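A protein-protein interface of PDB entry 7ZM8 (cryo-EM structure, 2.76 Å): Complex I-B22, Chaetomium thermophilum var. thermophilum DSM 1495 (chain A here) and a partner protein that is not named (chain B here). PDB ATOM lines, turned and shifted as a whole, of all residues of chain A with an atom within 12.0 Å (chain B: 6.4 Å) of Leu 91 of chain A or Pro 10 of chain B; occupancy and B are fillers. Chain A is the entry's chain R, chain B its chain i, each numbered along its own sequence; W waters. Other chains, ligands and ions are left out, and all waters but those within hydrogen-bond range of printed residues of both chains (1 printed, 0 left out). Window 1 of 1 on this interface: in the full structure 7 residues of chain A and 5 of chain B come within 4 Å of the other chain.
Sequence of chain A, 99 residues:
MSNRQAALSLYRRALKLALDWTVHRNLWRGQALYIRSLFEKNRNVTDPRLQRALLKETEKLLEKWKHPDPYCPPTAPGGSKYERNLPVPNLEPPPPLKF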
ATOM      1  N   ASN A  85      32.611  -4.267 -25.346  1.00  0.00           N
ATOM      2  CA  ASN A  85      31.997  -4.679 -24.074  1.00  0.00           C
ATOM      3  C   ASN A  85      32.532  -3.665 -23.087  1.00  0.00           C
ATOM      4  O   ASN A  85      33.249  -4.062 -22.160  1.00  0.00           O
ATOM      5  CB  ASN A  85      32.343  -6.140 -23.773  1.00  0.00           C
ATOM      6  CG  ASN A  85      31.404  -7.148 -24.399  1.00  0.00           C
ATOM      7  OD1 ASN A  85      30.200  -7.112 -24.172  1.00  0.00           O
ATOM      8  ND2 ASN A  85      31.953  -8.077 -25.158  1.00  0.00           N
ATOM      9  N   LEU A  86      32.188  -2.395 -23.303  1.00  0.00           N
ATOM     10  CA  LEU A  86      32.762  -1.328 -22.463  1.00  0.00           C
ATOM     11  C   LEU A  86      32.258  -1.529 -21.045  1.00  0.00           C
ATOM     12  O   LEU A  86      31.030  -1.606 -20.872  1.00  0.00           O
ATOM     13  CB  LEU A  86      32.359   0.034 -23.017  1.00  0.00           C
ATOM     14  CG  LEU A  86      33.327   0.673 -24.002  1.00  0.00           C
ATOM     15  CD1 LEU A  86      32.975   2.134 -24.204  1.00  0.00           C
ATOM     16  CD2 LEU A  86      34.758   0.534 -23.516  1.00  0.00           C
ATOM     17  N   PRO A  87      33.155  -1.589 -20.037  1.00  0.00           N
ATOM     18  CA  PRO A  87      32.748  -1.852 -18.659  1.00  0.00           C
ATOM     19  C   PRO A  87      31.923  -0.710 -18.061  1.00  0.00           C
ATOM     20  O   PRO A  87      32.101   0.391 -18.511  1.00  0.00           O
ATOM     21  CB  PRO A  87      34.091  -2.093 -17.960  1.00  0.00           C
ATOM     22  CG  PRO A  87      35.074  -1.277 -18.757  1.00  0.00           C
ATOM     23  CD  PRO A  87      34.601  -1.430 -20.183  1.00  0.00           C
ATOM     24  N   VAL A  88      31.046  -0.986 -17.091  1.00  0.00           N
ATOM     25  CA  VAL A  88      30.373   0.120 -16.407  1.00  0.00           C
ATOM     26  C   VAL A  88      31.425   1.038 -15.798  1.00  0.00           C
ATOM     27  O   VAL A  88      32.365   0.551 -15.142  1.00  0.00           O
ATOM     28  CB  VAL A  88      29.416  -0.418 -15.328  1.00  0.00           C
ATOM     29  CG1 VAL A  88      28.766   0.712 -14.573  1.00  0.00           C
ATOM     30  CG2 VAL A  88      28.363  -1.313 -15.955  1.00  0.00           C
ATOM     31  N   PRO A  89      31.345   2.353 -15.996  1.00  0.00           N
ATOM     32  CA  PRO A  89      32.342   3.261 -15.421  1.00  0.00           C
ATOM     33  C   PRO A  89      32.163   3.537 -13.938  1.00  0.00           C
ATOM     34  O   PRO A  89      32.791   4.464 -13.422  1.00  0.00           O
ATOM     35  CB  PRO A  89      32.139   4.552 -16.235  1.00  0.00           C
ATOM     36  CG  PRO A  89      31.147   4.220 -17.315  1.00  0.00           C
ATOM     37  CD  PRO A  89      30.368   3.066 -16.829  1.00  0.00           C
ATOM     38  N   ASN A  90      31.320   2.772 -13.248  1.00  0.00           N
ATOM     39  CA  ASN A  90      31.029   2.997 -11.836  1.00  0.00           C
ATOM     40  C   ASN A  90      30.557   1.663 -11.267  1.00  0.00           C
ATOM     41  O   ASN A  90      29.389   1.302 -11.425  1.00  0.00           O
ATOM     42  CB  ASN A  90      29.971   4.081 -11.681  1.00  0.00           C
ATOM     43  CG  ASN A  90      29.812   4.556 -10.258  1.00  0.00           C
ATOM     44  OD1 ASN A  90      29.913   3.783  -9.314  1.00  0.00           O
ATOM     45  ND2 ASN A  90      29.533   5.841 -10.102  1.00  0.00           N
ATOM     46  N   LEU A  91      31.454   0.946 -10.605  1.00  0.00           N
ATOM     47  CA  LEU A  91      31.114  -0.360 -10.061  1.00  0.00           C
ATOM     48  C   LEU A  91      30.692  -0.302  -8.602  1.00  0.00           C
ATOM     49  O   LEU A  91      30.389  -1.346  -8.017  1.00  0.00           O
ATOM     50  CB  LEU A  91      32.293  -1.323 -10.214  1.00  0.00           C
ATOM     51  CG  LEU A  91      32.959  -1.439 -11.584  1.00  0.00           C
ATOM     52  CD1 LEU A  91      33.999  -2.535 -11.543  1.00  0.00           C
ATOM     53  CD2 LEU A  91      31.945  -1.706 -12.669  1.00  0.00           C
ATOM     54  N   GLU A  92      30.666   0.872  -8.002  1.00  0.00           N
ATOM     55  CA  GLU A  92      30.261   0.967  -6.613  1.00  0.00           C
ATOM     56  C   GLU A  92      28.748   0.822  -6.483  1.00  0.00           C
ATOM     57  O   GLU A  92      27.996   1.255  -7.360  1.00  0.00           O
ATOM     58  CB  GLU A  92      30.703   2.297  -6.022  1.00  0.00           C
ATOM     59  CG  GLU A  92      32.208   2.452  -5.924  1.00  0.00           C
ATOM     60  CD  GLU A  92      32.830   1.488  -4.932  1.00  0.00           C
ATOM     61  OE1 GLU A  92      32.164   1.149  -3.932  1.00  0.00           O
ATOM     62  OE2 GLU A  92      33.984   1.069  -5.154  1.00  0.00           O
ATOM     63  N   PRO A  93      28.308   0.131  -5.389  1.00  0.00           N
ATOM     64  CA  PRO A  93      26.907  -0.146  -5.166  1.00  0.00           C
ATOM     65  C   PRO A  93      26.174   1.193  -5.117  1.00  0.00           C
ATOM     66  O   PRO A  93      26.798   2.194  -4.846  1.00  0.00           O
ATOM     67  CB  PRO A  93      26.920  -0.841  -3.810  1.00  0.00           C
ATOM     68  CG  PRO A  93      28.172  -1.624  -3.836  1.00  0.00           C
ATOM     69  CD  PRO A  93      29.105  -0.550  -4.326  1.00  0.00           C
ATOM     70  N   PRO A  94      24.855   1.249  -5.378  1.00  0.00           N
ATOM     71  CA  PRO A  94      24.175   2.527  -5.401  1.00  0.00           C
ATOM     72  C   PRO A  94      24.165   3.114  -3.979  1.00  0.00           C
ATOM     73  O   PRO A  94      24.156   2.360  -3.041  1.00  0.00           O
ATOM     74  CB  PRO A  94      22.793   2.160  -5.962  1.00  0.00           C
ATOM     75  CG  PRO A  94      22.961   0.791  -6.556  1.00  0.00           C
ATOM     76  CD  PRO A  94      23.974   0.125  -5.656  1.00  0.00           C
ATOM     77  N   PRO A  95      24.210   4.446  -3.790  1.00  0.00           N
ATOM     78  CA  PRO A  95      24.088   5.028  -2.452  1.00  0.00           C
ATOM     79  C   PRO A  95      22.689   4.694  -1.919  1.00  0.00           C
ATOM     80  O   PRO A  95      21.795   4.525  -2.711  1.00  0.00           O
ATOM     81  CB  PRO A  95      24.266   6.531  -2.643  1.00  0.00           C
ATOM     82  CG  PRO A  95      24.158   6.758  -4.136  1.00  0.00           C
ATOM     83  CD  PRO A  95      24.473   5.443  -4.816  1.00  0.00           C
ATOM     84  N   PRO B   8      35.430  -6.288 -15.742  1.00  0.00           N
ATOM     85  CA  PRO B   8      34.925  -5.925 -14.415  1.00  0.00           C
ATOM     86  C   PRO B   8      33.520  -5.351 -14.503  1.00  0.00           C
ATOM     87  O   PRO B   8      33.236  -4.486 -15.333  1.00  0.00           O
ATOM     88  CB  PRO B   8      35.927  -4.872 -13.934  1.00  0.00           C
ATOM     89  CG  PRO B   8      36.480  -4.298 -15.175  1.00  0.00           C
ATOM     90  CD  PRO B   8      36.519  -5.404 -16.180  1.00  0.00           C
ATOM     91  N   TYR B   9      32.645  -5.827 -13.633  1.00  0.00           N
ATOM     92  CA  TYR B   9      31.235  -5.480 -13.683  1.00  0.00           C
ATOM     93  C   TYR B   9      30.719  -5.248 -12.273  1.00  0.00           C
ATOM     94  O   TYR B   9      31.317  -5.721 -11.302  1.00  0.00           O
ATOM     95  CB  TYR B   9      30.417  -6.574 -14.380  1.00  0.00           C
ATOM     96  CG  TYR B   9      30.440  -7.906 -13.682  1.00  0.00           C
ATOM     97  CD1 TYR B   9      31.492  -8.782 -13.865  1.00  0.00           C
ATOM     98  CD2 TYR B   9      29.408  -8.289 -12.845  1.00  0.00           C
ATOM     99  CE1 TYR B   9      31.517  -9.995 -13.234  1.00  0.00           C
ATOM    100  CE2 TYR B   9      29.425  -9.500 -12.207  1.00  0.00           C
ATOM    101  CZ  TYR B   9      30.480 -10.349 -12.405  1.00  0.00           C
ATOM    102  OH  TYR B   9      30.509 -11.562 -11.771  1.00  0.00           O
ATOM    103  N   PRO B  10      29.615  -4.514 -12.131  1.00  0.00           N
ATOM    104  CA  PRO B  10      29.045  -4.280 -10.801  1.00  0.00           C
ATOM    105  C   PRO B  10      28.231  -5.467 -10.312  1.00  0.00           C
ATOM    106  O   PRO B  10      27.424  -6.044 -11.043  1.00  0.00           O
ATOM    107  CB  PRO B  10      28.157  -3.052 -11.020  1.00  0.00           C
ATOM    108  CG  PRO B  10      27.740  -3.166 -12.426  1.00  0.00           C
ATOM    109  CD  PRO B  10      28.882  -3.774 -13.173  1.00  0.00           C
ATOM    110  N   LYS B  11      28.439  -5.818  -9.049  1.00  0.00           N
ATOM    111  CA  LYS B  11      27.903  -7.043  -8.480  1.00  0.00           C
ATOM    112  C   LYS B  11      26.571  -6.847  -7.772  1.00  0.00           C
ATOM    113  O   LYS B  11      26.024  -7.807  -7.230  1.00  0.00           O
ATOM    114  CB  LYS B  11      28.925  -7.651  -7.528  1.00  0.00           C
ATOM    115  CG  LYS B  11      30.338  -7.586  -8.061  1.00  0.00           C
ATOM    116  CD  LYS B  11      30.640  -8.767  -8.953  1.00  0.00           C
ATOM    117  CE  LYS B  11      32.113  -8.832  -9.297  1.00  0.00           C
ATOM    118  NZ  LYS B  11      32.461  -7.906 -10.411  1.00  0.00           N
ATOM    119  N   HIS B  12      26.042  -5.631  -7.757  1.00  0.00           N
ATOM    120  CA  HIS B  12      24.727  -5.368  -7.202  1.00  0.00           C
ATOM    121  C   HIS B  12      23.632  -5.392  -8.254  1.00  0.00           C
ATOM    122  O   HIS B  12      22.457  -5.284  -7.901  1.00  0.00           O
ATOM    123  CB  HIS B  12      24.715  -4.010  -6.500  1.00  0.00           C
ATOM    124  CG  HIS B  12      24.781  -2.853  -7.443  1.00  0.00           C
ATOM    125  ND1 HIS B  12      25.967  -2.393  -7.967  1.00  0.00           N
ATOM    126  CD2 HIS B  12      23.808  -2.077  -7.971  1.00  0.00           C
ATOM    127  CE1 HIS B  12      25.721  -1.382  -8.778  1.00  0.00           C
ATOM    128  NE2 HIS B  12      24.418  -1.168  -8.798  1.00  0.00           N
ATOM    129  N   VAL B  13      23.988  -5.524  -9.525  1.00  0.00           N
ATOM    130  CA  VAL B  13      23.013  -5.463 -10.604  1.00  0.00           C
ATOM    131  C   VAL B  13      22.364  -6.829 -10.767  1.00  0.00           C
ATOM    132  O   VAL B  13      23.049  -7.836 -10.977  1.00  0.00           O
ATOM    133  CB  VAL B  13      23.672  -4.998 -11.911  1.00  0.00           C
ATOM    134  CG1 VAL B  13      22.709  -5.153 -13.066  1.00  0.00           C
ATOM    135  CG2 VAL B  13      24.125  -3.558 -11.793  1.00  0.00           C
ATOM    136  N   TRP B  20      26.633 -10.981 -16.155  1.00  0.00           N
ATOM    137  CA  TRP B  20      27.897 -11.029 -16.880  1.00  0.00           C
ATOM    138  C   TRP B  20      28.498 -12.421 -17.034  1.00  0.00           C
ATOM    139  O   TRP B  20      28.901 -12.785 -18.135  1.00  0.00           O
ATOM    140  CB  TRP B  20      28.899 -10.064 -16.253  1.00  0.00           C
ATOM    141  CG  TRP B  20      28.618  -8.640 -16.620  1.00  0.00           C
ATOM    142  CD1 TRP B  20      29.166  -7.966 -17.656  1.00  0.00           C
ATOM    143  CD2 TRP B  20      27.647  -7.763 -16.044  1.00  0.00           C
ATOM    144  NE1 TRP B  20      28.657  -6.701 -17.726  1.00  0.00           N
ATOM    145  CE2 TRP B  20      27.711  -6.554 -16.750  1.00  0.00           C
ATOM    146  CE3 TRP B  20      26.753  -7.870 -14.979  1.00  0.00           C
ATOM    147  CZ2 TRP B  20      26.921  -5.461 -16.430  1.00  0.00           C
ATOM    148  CZ3 TRP B  20      25.967  -6.786 -14.667  1.00  0.00           C
ATOM    149  CH2 TRP B  20      26.057  -5.599 -15.388  1.00  0.00           C
HETATM  150  O   HOH W   1      30.972  -4.094  -7.840  1.00  0.00           O
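O of Tyr 9 of chain B is in hydrogen-bond range of NZ of Lys 11 of chain B. The backbone NH (N) of Glu 92 of chain A lies within hydrogen-bond range of the side-chain amide oxygen (OD1) of Asn 90 of chain A.
Pro 87 of chain A touches Pro 8 of chain B (CB to O, 3.7 Å). CG2 of Val 88 of chain A touches CD of Pro 10 of chain B, at 3.8 Å. CD1 of Leu 91 of chain A touches CB of Pro 8 of chain B (3.9 Å). Tyr 9 of chain B touches Leu 91 of chain A (C to CD2, 3.8 Å). Pro 10 of chain B touches Leu 91 of chain A (N to CD2, 3.7 Å). His 12 of chain B touches Glu 92 of chain A (CE1 to O, 3.8 Å). His 12 of chain B touches Pro 93 of chain A. His 12 of chain B touches Pro 94 of chain A.
Hydrophobic or aromatic side chains of chain A that line the printed part of chain B: Pro 87, Val 88, Leu 91 and Pro 94. Printed residues of chain B that touch a printed residue of chain A: Pro 8, Tyr 9, Pro 10 and His 12. Hydrophobic or aromatic side chains of chain B that line the printed part of chain A: Pro 8, Pro 10 and His 12.
Leu 91 of chain A touches just these residues of chain B: Pro 8 (3.9 Å), Tyr 9 (3.8 Å) and Pro 10 (3.7 Å). Pro 10 of chain B touches just these residues of chain A: Val 88 and Leu 91. Tyr 9 of chain B touches just one residue of chain A: Leu 91 (3.8 Å). No residue of chain A comes within 4 Å of Lys 11 of chain B. Of chain A, only Glu 92, Pro 93 and Pro 94 come within 4 Å of His 12 of chain B. Of the printed residues of chain B, Pro 87 of chain A touches Pro 8 (3.7 Å). Of the printed residues of chain B, Glu 92 of chain A touches His 12 (3.8 Å). Of the printed residues of chain B, Val 88 of chain A touches Pro 10. Of the printed residues of chain B, Pro 93 of chain A touches His 12. Pro 89 of chain A touches none of the printed residues of chain B. The nearest residue of chain A that does not touch Pro 10 of chain B is Asn 90 of chain A (4.5 Å).
Water W1 bridges O of Leu 91 of chain A and N of Lys 11 of chain B.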
